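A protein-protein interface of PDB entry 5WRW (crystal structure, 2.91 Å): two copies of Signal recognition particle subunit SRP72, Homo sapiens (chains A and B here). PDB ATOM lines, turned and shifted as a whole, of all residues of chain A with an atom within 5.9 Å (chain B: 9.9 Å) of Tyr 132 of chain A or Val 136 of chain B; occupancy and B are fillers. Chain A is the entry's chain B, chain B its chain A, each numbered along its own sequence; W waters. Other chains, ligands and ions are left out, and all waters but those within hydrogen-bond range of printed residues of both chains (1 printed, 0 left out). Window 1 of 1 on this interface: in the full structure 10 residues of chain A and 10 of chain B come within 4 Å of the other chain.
The side-chain carboxylate (OE2) of Glu 113 of chain A is in salt-bridge range of the guanidinium group (NH1) of Arg 137 of chain B (3.6 Å). OE1 of Gln 117 of chain A lies within hydrogen-bond range of NH1 of Arg 133 of chain B (3.1 Å). The guanidinium group (NH2) of Arg 137 of chain B sits at hydrogen-bond distance from the side-chain amide oxygen (OE1) of Gln 117 of chain A (2.8 Å). NH1 of Arg 137 of chain B lies within hydrogen-bond range of OH of Tyr 132 of chain A (2.9 Å).
OD1 of Asn 138 of chain B sits close to O of Val 136 of chain B (3.3 Å). SG of Cys 128 of chain A is in hydrogen-bond range of O of Gly 116 of chain A. The side-chain carboxylate (OE2) of Glu 113 of chain B is in hydrogen-bond range of the side-chain hydroxyl (OH) of Tyr 132 of chain B (3.3 Å). O of Gly 116 of chain B is in hydrogen-bond range of SG of Cys 128 of chain B (3.6 Å).
Among the printed residues, merely in contact across the chains: Arg 137 of chain A with Glu 113 of chain B (3.3 Å), Tyr 120 of chain A with Arg 133 of chain B (3.3 Å), Val 136 of chain A with Val 136 of chain B (3.4 Å), Arg 133 of chain A with Tyr 120 of chain B (3.4 Å), Glu 113 of chain A with Val 136 of chain B (3.5 Å), Tyr 132 of chain A with Arg 133 of chain B (3.5 Å), Tyr 120 of chain A with Leu 129 of chain B (3.7 Å), Arg 137 of chain A with Tyr 132 of chain B (3.7 Å), Arg 133 of chain A with Tyr 132 of chain B (3.7 Å), Tyr 132 of chain A with Val 136 of chain B (3.7 Å), Val 136 of chain A with Glu 113 of chain B (3.8 Å), Leu 129 of chain A with Cys 128 of chain B (3.8 Å), Val 136 of chain A with Tyr 132 of chain B (3.9 Å), Leu 129 of chain A with Tyr 120 of chain B (3.9 Å), Cys 128 of chain A with Leu 129 of chain B (3.9 Å) and Leu 129 of chain A with Tyr 125 of chain B (3.9 Å).
Of chain B, only Arg 133, Val 136 and Arg 137 come within 4 Å of Tyr 132 of chain A. Gly 116 of chain A touches none of the printed residues of chain B. No residue of chain B comes within 4 Å of Val 131 of chain A. Of the printed residues of chain B, Leu 129 of chain A touches Tyr 120, Tyr 125 and Cys 128. Of the printed residues of chain B, Cys 128 of chain A touches Leu 129. Of the printed residues of chain B, Val 136 of chain A touches Glu 113, Tyr 132 and Val 136. The nearest printed residue of chain B that does not touch Arg 137 of chain A is Tyr 120 of chain B (6.7 Å).
Of the 16 printed residues of chain A, 9 touch a printed residue of chain B. Printed residues of chain A that touch a printed residue of chain B: Glu 113, Gln 117, Tyr 120, Cys 128, Leu 129, Tyr 132, Arg 133, Val 136 and Arg 137. Hydrophobic or aromatic side chains of chain A that line the printed part of chain B: Tyr 120, Leu 129, Tyr 132 and Val 136. Among the printed residues, Asp or Glu carboxylates within 4 Å of a Lys or Arg side-chain nitrogen of the other chain: Glu 113 of chain A with Arg 137 of chain B.
Tyr 120 of chain A touches Leu 129 of chain B, and with the chains exchanged Leu 129 of chain A touches Tyr 120 of chain B. Tyr 132 of chain A touches Val 136 of chain B, and with the chains exchanged Val 136 of chain A touches Tyr 132 of chain B. Tyr 132 of chain A touches Arg 137 of chain B, and with the chains exchanged Arg 137 of chain A touches Tyr 132 of chain B. Val 136 of chain B touches its own counterpart, Val 136 of chain A. Of the 20 pairs that touch across the chains among the printed residues, 17 have their exchanged pair printed and touching as well.
Water W1 bridges the guanidinium group (NH1) of Arg 133 of chain A and the side-chain hydroxyl (OH) of Tyr 120 of chain B.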
ATOM      1  N   GLU A 113       4.951  22.846   0.215  1.00  0.00           N
ATOM      2  CA  GLU A 113       5.828  22.703   1.379  1.00  0.00           C
ATOM      3  C   GLU A 113       7.282  23.091   1.097  1.00  0.00           C
ATOM      4  O   GLU A 113       7.963  23.558   2.004  1.00  0.00           O
ATOM      5  CB  GLU A 113       5.783  21.276   1.931  1.00  0.00           C
ATOM      6  CG  GLU A 113       6.546  21.084   3.241  1.00  0.00           C
ATOM      7  CD  GLU A 113       6.428  19.679   3.811  1.00  0.00           C
ATOM      8  OE1 GLU A 113       5.850  18.783   3.148  1.00  0.00           O
ATOM      9  OE2 GLU A 113       6.930  19.466   4.935  1.00  0.00           O
ATOM     10  N   LEU A 114       7.751  22.881  -0.137  1.00  0.00           N
ATOM     11  CA  LEU A 114       9.130  23.232  -0.534  1.00  0.00           C
ATOM     12  C   LEU A 114       9.252  24.715  -0.840  1.00  0.00           C
ATOM     13  O   LEU A 114      10.298  25.320  -0.594  1.00  0.00           O
ATOM     14  CB  LEU A 114       9.572  22.420  -1.758  1.00  0.00           C
ATOM     15  CG  LEU A 114      11.020  22.552  -2.235  1.00  0.00           C
ATOM     16  CD1 LEU A 114      11.994  21.974  -1.229  1.00  0.00           C
ATOM     17  CD2 LEU A 114      11.177  21.851  -3.571  1.00  0.00           C
ATOM     18  N   GLY A 116       7.453  26.877   0.726  1.00  0.00           N
ATOM     19  CA  GLY A 116       7.504  27.413   2.083  1.00  0.00           C
ATOM     20  C   GLY A 116       8.932  27.467   2.592  1.00  0.00           C
ATOM     21  O   GLY A 116       9.437  28.525   2.974  1.00  0.00           O
ATOM     22  N   GLN A 117       9.588  26.316   2.545  1.00  0.00           N
ATOM     23  CA  GLN A 117      10.967  26.183   2.989  1.00  0.00           C
ATOM     24  C   GLN A 117      11.925  27.117   2.279  1.00  0.00           C
ATOM     25  O   GLN A 117      12.820  27.673   2.905  1.00  0.00           O
ATOM     26  CB  GLN A 117      11.466  24.739   2.843  1.00  0.00           C
ATOM     27  CG  GLN A 117      11.676  24.033   4.176  1.00  0.00           C
ATOM     28  CD  GLN A 117      12.807  24.607   5.063  1.00  0.00           C
ATOM     29  OE1 GLN A 117      12.907  24.225   6.234  1.00  0.00           O
ATOM     30  NE2 GLN A 117      13.649  25.512   4.521  1.00  0.00           N
ATOM     31  N   TYR A 120      11.278  30.487   3.673  1.00  0.00           N
ATOM     32  CA  TYR A 120      11.876  30.541   5.024  1.00  0.00           C
ATOM     33  C   TYR A 120      13.375  30.793   4.978  1.00  0.00           C
ATOM     34  O   TYR A 120      13.899  31.610   5.735  1.00  0.00           O
ATOM     35  CB  TYR A 120      11.620  29.264   5.830  1.00  0.00           C
ATOM     36  CG  TYR A 120      11.861  29.444   7.315  1.00  0.00           C
ATOM     37  CD1 TYR A 120      10.881  30.002   8.129  1.00  0.00           C
ATOM     38  CD2 TYR A 120      13.060  29.072   7.902  1.00  0.00           C
ATOM     39  CE1 TYR A 120      11.090  30.187   9.487  1.00  0.00           C
ATOM     40  CE2 TYR A 120      13.285  29.247   9.263  1.00  0.00           C
ATOM     41  CZ  TYR A 120      12.290  29.804  10.056  1.00  0.00           C
ATOM     42  OH  TYR A 120      12.463  29.986  11.413  1.00  0.00           O
ATOM     43  N   GLU A 127       5.290  35.783   3.302  1.00  0.00           N
ATOM     44  CA  GLU A 127       4.904  34.930   2.172  1.00  0.00           C
ATOM     45  C   GLU A 127       4.872  33.479   2.622  1.00  0.00           C
ATOM     46  O   GLU A 127       3.952  32.734   2.276  1.00  0.00           O
ATOM     47  CB  GLU A 127       5.867  35.101   0.996  1.00  0.00           C
ATOM     48  CG  GLU A 127       5.803  36.465   0.314  1.00  0.00           C
ATOM     49  CD  GLU A 127       7.036  36.760  -0.539  1.00  0.00           C
ATOM     50  OE1 GLU A 127       7.923  37.510  -0.064  1.00  0.00           O
ATOM     51  OE2 GLU A 127       7.131  36.231  -1.672  1.00  0.00           O
ATOM     52  N   CYS A 128       5.882  33.119   3.418  1.00  0.00           N
ATOM     53  CA  CYS A 128       6.052  31.795   4.019  1.00  0.00           C
ATOM     54  C   CYS A 128       4.877  31.440   4.928  1.00  0.00           C
ATOM     55  O   CYS A 128       4.340  30.350   4.832  1.00  0.00           O
ATOM     56  CB  CYS A 128       7.374  31.776   4.792  1.00  0.00           C
ATOM     57  SG  CYS A 128       7.868  30.217   5.541  1.00  0.00           S
ATOM     58  N   LEU A 129       4.458  32.364   5.788  1.00  0.00           N
ATOM     59  CA  LEU A 129       3.282  32.113   6.660  1.00  0.00           C
ATOM     60  C   LEU A 129       2.039  31.725   5.842  1.00  0.00           C
ATOM     61  O   LEU A 129       1.363  30.735   6.148  1.00  0.00           O
ATOM     62  CB  LEU A 129       2.939  33.334   7.531  1.00  0.00           C
ATOM     63  CG  LEU A 129       2.553  33.101   8.998  1.00  0.00           C
ATOM     64  CD1 LEU A 129       1.792  34.304   9.566  1.00  0.00           C
ATOM     65  CD2 LEU A 129       1.758  31.825   9.201  1.00  0.00           C
ATOM     66  N   ALA A 130       1.765  32.515   4.801  1.00  0.00           N
ATOM     67  CA  ALA A 130       0.633  32.294   3.895  1.00  0.00           C
ATOM     68  C   ALA A 130       0.657  30.899   3.274  1.00  0.00           C
ATOM     69  O   ALA A 130      -0.393  30.245   3.188  1.00  0.00           O
ATOM     70  CB  ALA A 130       0.622  33.341   2.797  1.00  0.00           C
ATOM     71  N   VAL A 131       1.852  30.458   2.861  1.00  0.00           N
ATOM     72  CA  VAL A 131       2.054  29.142   2.258  1.00  0.00           C
ATOM     73  C   VAL A 131       1.777  28.051   3.278  1.00  0.00           C
ATOM     74  O   VAL A 131       1.049  27.099   2.990  1.00  0.00           O
ATOM     75  CB  VAL A 131       3.485  28.998   1.697  1.00  0.00           C
ATOM     76  CG1 VAL A 131       3.828  27.555   1.342  1.00  0.00           C
ATOM     77  CG2 VAL A 131       3.674  29.909   0.483  1.00  0.00           C
ATOM     78  N   TYR A 132       2.351  28.199   4.468  1.00  0.00           N
ATOM     79  CA  TYR A 132       2.167  27.204   5.530  1.00  0.00           C
ATOM     80  C   TYR A 132       0.732  27.161   6.071  1.00  0.00           C
ATOM     81  O   TYR A 132       0.253  26.086   6.406  1.00  0.00           O
ATOM     82  CB  TYR A 132       3.213  27.370   6.660  1.00  0.00           C
ATOM     83  CG  TYR A 132       4.527  26.684   6.340  1.00  0.00           C
ATOM     84  CD1 TYR A 132       4.659  25.301   6.474  1.00  0.00           C
ATOM     85  CD2 TYR A 132       5.618  27.402   5.866  1.00  0.00           C
ATOM     86  CE1 TYR A 132       5.841  24.658   6.158  1.00  0.00           C
ATOM     87  CE2 TYR A 132       6.809  26.765   5.541  1.00  0.00           C
ATOM     88  CZ  TYR A 132       6.915  25.396   5.687  1.00  0.00           C
ATOM     89  OH  TYR A 132       8.099  24.776   5.385  1.00  0.00           O
ATOM     90  N   ARG A 133       0.048  28.309   6.143  1.00  0.00           N
ATOM     91  CA  ARG A 133      -1.362  28.334   6.583  1.00  0.00           C
ATOM     92  C   ARG A 133      -2.267  27.725   5.531  1.00  0.00           C
ATOM     93  O   ARG A 133      -3.072  26.855   5.839  1.00  0.00           O
ATOM     94  CB  ARG A 133      -1.837  29.747   6.904  1.00  0.00           C
ATOM     95  CG  ARG A 133      -1.250  30.275   8.189  1.00  0.00           C
ATOM     96  CD  ARG A 133      -1.689  31.701   8.485  1.00  0.00           C
ATOM     97  NE  ARG A 133      -2.771  31.704   9.464  1.00  0.00           N
ATOM     98  CZ  ARG A 133      -4.029  32.081   9.248  1.00  0.00           C
ATOM     99  NH1 ARG A 133      -4.448  32.543   8.061  1.00  0.00           N
ATOM    100  NH2 ARG A 133      -4.888  32.008  10.253  1.00  0.00           N
ATOM    101  N   ASP A 134      -2.124  28.178   4.290  1.00  0.00           N
ATOM    102  CA  ASP A 134      -2.809  27.549   3.170  1.00  0.00           C
ATOM    103  C   ASP A 134      -2.687  26.025   3.291  1.00  0.00           C
ATOM    104  O   ASP A 134      -3.684  25.317   3.359  1.00  0.00           O
ATOM    105  CB  ASP A 134      -2.215  28.036   1.845  1.00  0.00           C
ATOM    106  CG  ASP A 134      -2.830  27.356   0.634  1.00  0.00           C
ATOM    107  OD1 ASP A 134      -4.041  27.062   0.652  1.00  0.00           O
ATOM    108  OD2 ASP A 134      -2.096  27.120  -0.346  1.00  0.00           O
ATOM    109  N   LEU A 135      -1.458  25.544   3.377  1.00  0.00           N
ATOM    110  CA  LEU A 135      -1.191  24.114   3.464  1.00  0.00           C
ATOM    111  C   LEU A 135      -1.973  23.397   4.565  1.00  0.00           C
ATOM    112  O   LEU A 135      -2.522  22.328   4.328  1.00  0.00           O
ATOM    113  CB  LEU A 135       0.303  23.872   3.668  1.00  0.00           C
ATOM    114  CG  LEU A 135       0.905  22.796   2.782  1.00  0.00           C
ATOM    115  CD1 LEU A 135       2.385  23.095   2.594  1.00  0.00           C
ATOM    116  CD2 LEU A 135       0.667  21.416   3.382  1.00  0.00           C
ATOM    117  N   VAL A 136      -2.027  23.992   5.754  1.00  0.00           N
ATOM    118  CA  VAL A 136      -2.678  23.380   6.926  1.00  0.00           C
ATOM    119  C   VAL A 136      -4.199  23.546   6.910  1.00  0.00           C
ATOM    120  O   VAL A 136      -4.929  22.720   7.459  1.00  0.00           O
ATOM    121  CB  VAL A 136      -2.061  23.922   8.245  1.00  0.00           C
ATOM    122  CG1 VAL A 136      -2.842  23.490   9.489  1.00  0.00           C
ATOM    123  CG2 VAL A 136      -0.612  23.454   8.359  1.00  0.00           C
ATOM    124  N   ARG A 137      -4.682  24.601   6.270  1.00  0.00           N
ATOM    125  CA  ARG A 137      -6.113  24.901   6.242  1.00  0.00           C
ATOM    126  C   ARG A 137      -6.595  24.745   4.782  1.00  0.00           C
ATOM    127  O   ARG A 137      -7.228  25.639   4.218  1.00  0.00           O
ATOM    128  CB  ARG A 137      -6.322  26.305   6.838  1.00  0.00           C
ATOM    129  CG  ARG A 137      -5.407  26.587   8.047  1.00  0.00           C
ATOM    130  CD  ARG A 137      -5.997  27.535   9.078  1.00  0.00           C
ATOM    131  NE  ARG A 137      -6.583  28.720   8.450  1.00  0.00           N
ATOM    132  CZ  ARG A 137      -7.675  29.368   8.874  1.00  0.00           C
ATOM    133  NH1 ARG A 137      -8.358  28.978   9.959  1.00  0.00           N
ATOM    134  NH2 ARG A 137      -8.102  30.432   8.197  1.00  0.00           N
ATOM    135  N   ASP B 109      -3.360  17.980  17.817  1.00  0.00           N
ATOM    136  CA  ASP B 109      -3.096  18.698  16.567  1.00  0.00           C
ATOM    137  C   ASP B 109      -4.092  19.824  16.341  1.00  0.00           C
ATOM    138  O   ASP B 109      -3.689  20.956  16.084  1.00  0.00           O
ATOM    139  CB  ASP B 109      -3.067  17.751  15.353  1.00  0.00           C
ATOM    140  CG  ASP B 109      -1.684  17.142  15.103  1.00  0.00           C
ATOM    141  OD1 ASP B 109      -0.748  17.341  15.924  1.00  0.00           O
ATOM    142  OD2 ASP B 109      -1.543  16.455  14.066  1.00  0.00           O
ATOM    143  N   LYS B 112      -3.330  22.540  18.486  1.00  0.00           N
ATOM    144  CA  LYS B 112      -2.136  23.226  17.977  1.00  0.00           C
ATOM    145  C   LYS B 112      -2.519  24.196  16.850  1.00  0.00           C
ATOM    146  O   LYS B 112      -2.057  25.334  16.830  1.00  0.00           O
ATOM    147  CB  LYS B 112      -1.084  22.207  17.486  1.00  0.00           C
ATOM    148  CG  LYS B 112       0.377  22.587  17.721  1.00  0.00           C
ATOM    149  CD  LYS B 112       1.244  21.341  17.860  1.00  0.00           C
ATOM    150  CE  LYS B 112       1.126  20.708  19.252  1.00  0.00           C
ATOM    151  NZ  LYS B 112       1.253  19.219  19.268  1.00  0.00           N
ATOM    152  N   GLU B 113      -3.358  23.734  15.925  1.00  0.00           N
ATOM    153  CA  GLU B 113      -3.838  24.568  14.806  1.00  0.00           C
ATOM    154  C   GLU B 113      -4.641  25.782  15.285  1.00  0.00           C
ATOM    155  O   GLU B 113      -4.577  26.842  14.662  1.00  0.00           O
ATOM    156  CB  GLU B 113      -4.618  23.722  13.776  1.00  0.00           C
ATOM    157  CG  GLU B 113      -6.017  24.205  13.385  1.00  0.00           C
ATOM    158  CD  GLU B 113      -6.048  24.923  12.055  1.00  0.00           C
ATOM    159  OE1 GLU B 113      -6.191  24.203  11.030  1.00  0.00           O
ATOM    160  OE2 GLU B 113      -5.949  26.184  12.046  1.00  0.00           O
ATOM    161  N   GLY B 116      -2.196  28.394  16.664  1.00  0.00           N
ATOM    162  CA  GLY B 116      -1.660  29.174  15.558  1.00  0.00           C
ATOM    163  C   GLY B 116      -2.587  30.301  15.167  1.00  0.00           C
ATOM    164  O   GLY B 116      -2.175  31.465  15.083  1.00  0.00           O
ATOM    165  N   TYR B 120      -2.131  34.315  15.215  1.00  0.00           N
ATOM    166  CA  TYR B 120      -2.333  35.124  14.000  1.00  0.00           C
ATOM    167  C   TYR B 120      -3.260  36.302  14.287  1.00  0.00           C
ATOM    168  O   TYR B 120      -3.032  37.416  13.806  1.00  0.00           O
ATOM    169  CB  TYR B 120      -2.937  34.249  12.909  1.00  0.00           C
ATOM    170  CG  TYR B 120      -3.032  34.844  11.521  1.00  0.00           C
ATOM    171  CD1 TYR B 120      -1.929  34.860  10.667  1.00  0.00           C
ATOM    172  CD2 TYR B 120      -4.245  35.304  11.025  1.00  0.00           C
ATOM    173  CE1 TYR B 120      -2.028  35.367   9.379  1.00  0.00           C
ATOM    174  CE2 TYR B 120      -4.352  35.799   9.742  1.00  0.00           C
ATOM    175  CZ  TYR B 120      -3.245  35.834   8.933  1.00  0.00           C
ATOM    176  OH  TYR B 120      -3.367  36.329   7.670  1.00  0.00           O
ATOM    177  N   TYR B 125       3.075  37.025  14.652  1.00  0.00           N
ATOM    178  CA  TYR B 125       3.267  36.298  13.396  1.00  0.00           C
ATOM    179  C   TYR B 125       4.416  35.324  13.417  1.00  0.00           C
ATOM    180  O   TYR B 125       4.306  34.243  12.845  1.00  0.00           O
ATOM    181  CB  TYR B 125       3.414  37.259  12.209  1.00  0.00           C
ATOM    182  CG  TYR B 125       2.179  38.102  11.949  1.00  0.00           C
ATOM    183  CD1 TYR B 125       0.943  37.507  11.699  1.00  0.00           C
ATOM    184  CD2 TYR B 125       2.251  39.491  11.944  1.00  0.00           C
ATOM    185  CE1 TYR B 125      -0.189  38.275  11.459  1.00  0.00           C
ATOM    186  CE2 TYR B 125       1.132  40.270  11.711  1.00  0.00           C
ATOM    187  CZ  TYR B 125      -0.085  39.664  11.468  1.00  0.00           C
ATOM    188  OH  TYR B 125      -1.180  40.450  11.237  1.00  0.00           O
ATOM    189  N   CYS B 128       3.347  32.390  15.349  1.00  0.00           N
ATOM    190  CA  CYS B 128       2.375  31.753  14.473  1.00  0.00           C
ATOM    191  C   CYS B 128       3.105  30.884  13.423  1.00  0.00           C
ATOM    192  O   CYS B 128       2.837  29.685  13.302  1.00  0.00           O
ATOM    193  CB  CYS B 128       1.473  32.828  13.826  1.00  0.00           C
ATOM    194  SG  CYS B 128       0.254  32.260  12.619  1.00  0.00           S
ATOM    195  N   LEU B 129       4.054  31.480  12.707  1.00  0.00           N
ATOM    196  CA  LEU B 129       4.775  30.762  11.638  1.00  0.00           C
ATOM    197  C   LEU B 129       5.412  29.476  12.195  1.00  0.00           C
ATOM    198  O   LEU B 129       5.287  28.409  11.608  1.00  0.00           O
ATOM    199  CB  LEU B 129       5.863  31.647  11.014  1.00  0.00           C
ATOM    200  CG  LEU B 129       6.330  31.441   9.565  1.00  0.00           C
ATOM    201  CD1 LEU B 129       7.795  31.827   9.378  1.00  0.00           C
ATOM    202  CD2 LEU B 129       6.113  30.041   9.057  1.00  0.00           C
ATOM    203  N   ALA B 130       6.063  29.600  13.350  1.00  0.00           N
ATOM    204  CA  ALA B 130       6.643  28.453  14.048  1.00  0.00           C
ATOM    205  C   ALA B 130       5.611  27.356  14.269  1.00  0.00           C
ATOM    206  O   ALA B 130       5.878  26.198  13.967  1.00  0.00           O
ATOM    207  CB  ALA B 130       7.250  28.879  15.372  1.00  0.00           C
ATOM    208  N   VAL B 131       4.425  27.728  14.753  1.00  0.00           N
ATOM    209  CA  VAL B 131       3.359  26.749  15.004  1.00  0.00           C
ATOM    210  C   VAL B 131       2.951  26.031  13.719  1.00  0.00           C
ATOM    211  O   VAL B 131       2.840  24.806  13.712  1.00  0.00           O
ATOM    212  CB  VAL B 131       2.111  27.379  15.675  1.00  0.00           C
ATOM    213  CG1 VAL B 131       0.941  26.387  15.720  1.00  0.00           C
ATOM    214  CG2 VAL B 131       2.449  27.877  17.081  1.00  0.00           C
ATOM    215  N   TYR B 132       2.728  26.783  12.645  1.00  0.00           N
ATOM    216  CA  TYR B 132       2.280  26.177  11.386  1.00  0.00           C
ATOM    217  C   TYR B 132       3.370  25.307  10.734  1.00  0.00           C
ATOM    218  O   TYR B 132       3.055  24.278  10.138  1.00  0.00           O
ATOM    219  CB  TYR B 132       1.698  27.235  10.420  1.00  0.00           C
ATOM    220  CG  TYR B 132       0.267  27.642  10.776  1.00  0.00           C
ATOM    221  CD1 TYR B 132      -0.801  26.809  10.462  1.00  0.00           C
ATOM    222  CD2 TYR B 132      -0.020  28.848  11.447  1.00  0.00           C
ATOM    223  CE1 TYR B 132      -2.106  27.149  10.791  1.00  0.00           C
ATOM    224  CE2 TYR B 132      -1.336  29.193  11.779  1.00  0.00           C
ATOM    225  CZ  TYR B 132      -2.375  28.335  11.443  1.00  0.00           C
ATOM    226  OH  TYR B 132      -3.685  28.631  11.741  1.00  0.00           O
ATOM    227  N   ARG B 133       4.644  25.680  10.886  1.00  0.00           N
ATOM    228  CA  ARG B 133       5.730  24.853  10.356  1.00  0.00           C
ATOM    229  C   ARG B 133       5.803  23.580  11.144  1.00  0.00           C
ATOM    230  O   ARG B 133       5.759  22.515  10.563  1.00  0.00           O
ATOM    231  CB  ARG B 133       7.079  25.534  10.415  1.00  0.00           C
ATOM    232  CG  ARG B 133       7.138  26.855   9.694  1.00  0.00           C
ATOM    233  CD  ARG B 133       8.292  26.933   8.719  1.00  0.00           C
ATOM    234  NE  ARG B 133       9.582  26.796   9.383  1.00  0.00           N
ATOM    235  CZ  ARG B 133      10.706  26.401   8.785  1.00  0.00           C
ATOM    236  NH1 ARG B 133      10.743  26.086   7.481  1.00  0.00           N
ATOM    237  NH2 ARG B 133      11.819  26.314   9.506  1.00  0.00           N
ATOM    238  N   ASP B 134       5.878  23.688  12.467  1.00  0.00           N
ATOM    239  CA  ASP B 134       5.864  22.507  13.337  1.00  0.00           C
ATOM    240  C   ASP B 134       4.698  21.575  12.980  1.00  0.00           C
ATOM    241  O   ASP B 134       4.890  20.368  12.889  1.00  0.00           O
ATOM    242  CB  ASP B 134       5.822  22.903  14.819  1.00  0.00           C
ATOM    243  CG  ASP B 134       5.308  21.781  15.717  1.00  0.00           C
ATOM    244  OD1 ASP B 134       5.852  20.654  15.656  1.00  0.00           O
ATOM    245  OD2 ASP B 134       4.346  22.027  16.487  1.00  0.00           O
ATOM    246  N   LEU B 135       3.508  22.137  12.762  1.00  0.00           N
ATOM    247  CA  LEU B 135       2.345  21.335  12.363  1.00  0.00           C
ATOM    248  C   LEU B 135       2.558  20.579  11.055  1.00  0.00           C
ATOM    249  O   LEU B 135       2.127  19.442  10.944  1.00  0.00           O
ATOM    250  CB  LEU B 135       1.060  22.175  12.268  1.00  0.00           C
ATOM    251  CG  LEU B 135       0.101  22.149  13.459  1.00  0.00           C
ATOM    252  CD1 LEU B 135      -1.080  23.040  13.130  1.00  0.00           C
ATOM    253  CD2 LEU B 135      -0.396  20.749  13.793  1.00  0.00           C
ATOM    254  N   VAL B 136       3.208  21.205  10.076  1.00  0.00           N
ATOM    255  CA  VAL B 136       3.452  20.561   8.775  1.00  0.00           C
ATOM    256  C   VAL B 136       4.561  19.500   8.811  1.00  0.00           C
ATOM    257  O   VAL B 136       4.447  18.502   8.101  1.00  0.00           O
ATOM    258  CB  VAL B 136       3.700  21.595   7.654  1.00  0.00           C
ATOM    259  CG1 VAL B 136       4.066  20.906   6.342  1.00  0.00           C
ATOM    260  CG2 VAL B 136       2.450  22.435   7.452  1.00  0.00           C
ATOM    261  N   ARG B 137       5.609  19.694   9.620  1.00  0.00           N
ATOM    262  CA  ARG B 137       6.632  18.632   9.815  1.00  0.00           C
ATOM    263  C   ARG B 137       6.178  17.582  10.848  1.00  0.00           C
ATOM    264  O   ARG B 137       6.773  16.526  10.920  1.00  0.00           O
ATOM    265  CB  ARG B 137       8.036  19.143  10.229  1.00  0.00           C
ATOM    266  CG  ARG B 137       8.270  20.645  10.351  1.00  0.00           C
ATOM    267  CD  ARG B 137       8.223  21.402   9.022  1.00  0.00           C
ATOM    268  NE  ARG B 137       9.568  21.682   8.527  1.00  0.00           N
ATOM    269  CZ  ARG B 137       9.875  22.023   7.276  1.00  0.00           C
ATOM    270  NH1 ARG B 137       8.936  22.165   6.330  1.00  0.00           N
ATOM    271  NH2 ARG B 137      11.156  22.224   6.976  1.00  0.00           N
ATOM    272  N   ASN B 138       5.154  17.890  11.648  1.00  0.00           N
ATOM    273  CA  ASN B 138       4.675  17.051  12.771  1.00  0.00           C
ATOM    274  C   ASN B 138       5.713  16.914  13.901  1.00  0.00           C
ATOM    275  O   ASN B 138       6.654  17.711  14.012  1.00  0.00           O
ATOM    276  CB  ASN B 138       4.194  15.664  12.306  1.00  0.00           C
ATOM    277  CG  ASN B 138       3.063  15.736  11.286  1.00  0.00           C
ATOM    278  OD1 ASN B 138       3.147  16.447  10.285  1.00  0.00           O
ATOM    279  ND2 ASN B 138       2.005  14.975  11.529  1.00  0.00           N
HETATM  280  O   HOH W   1      -6.033  34.868   6.204  1.00  0.00           O
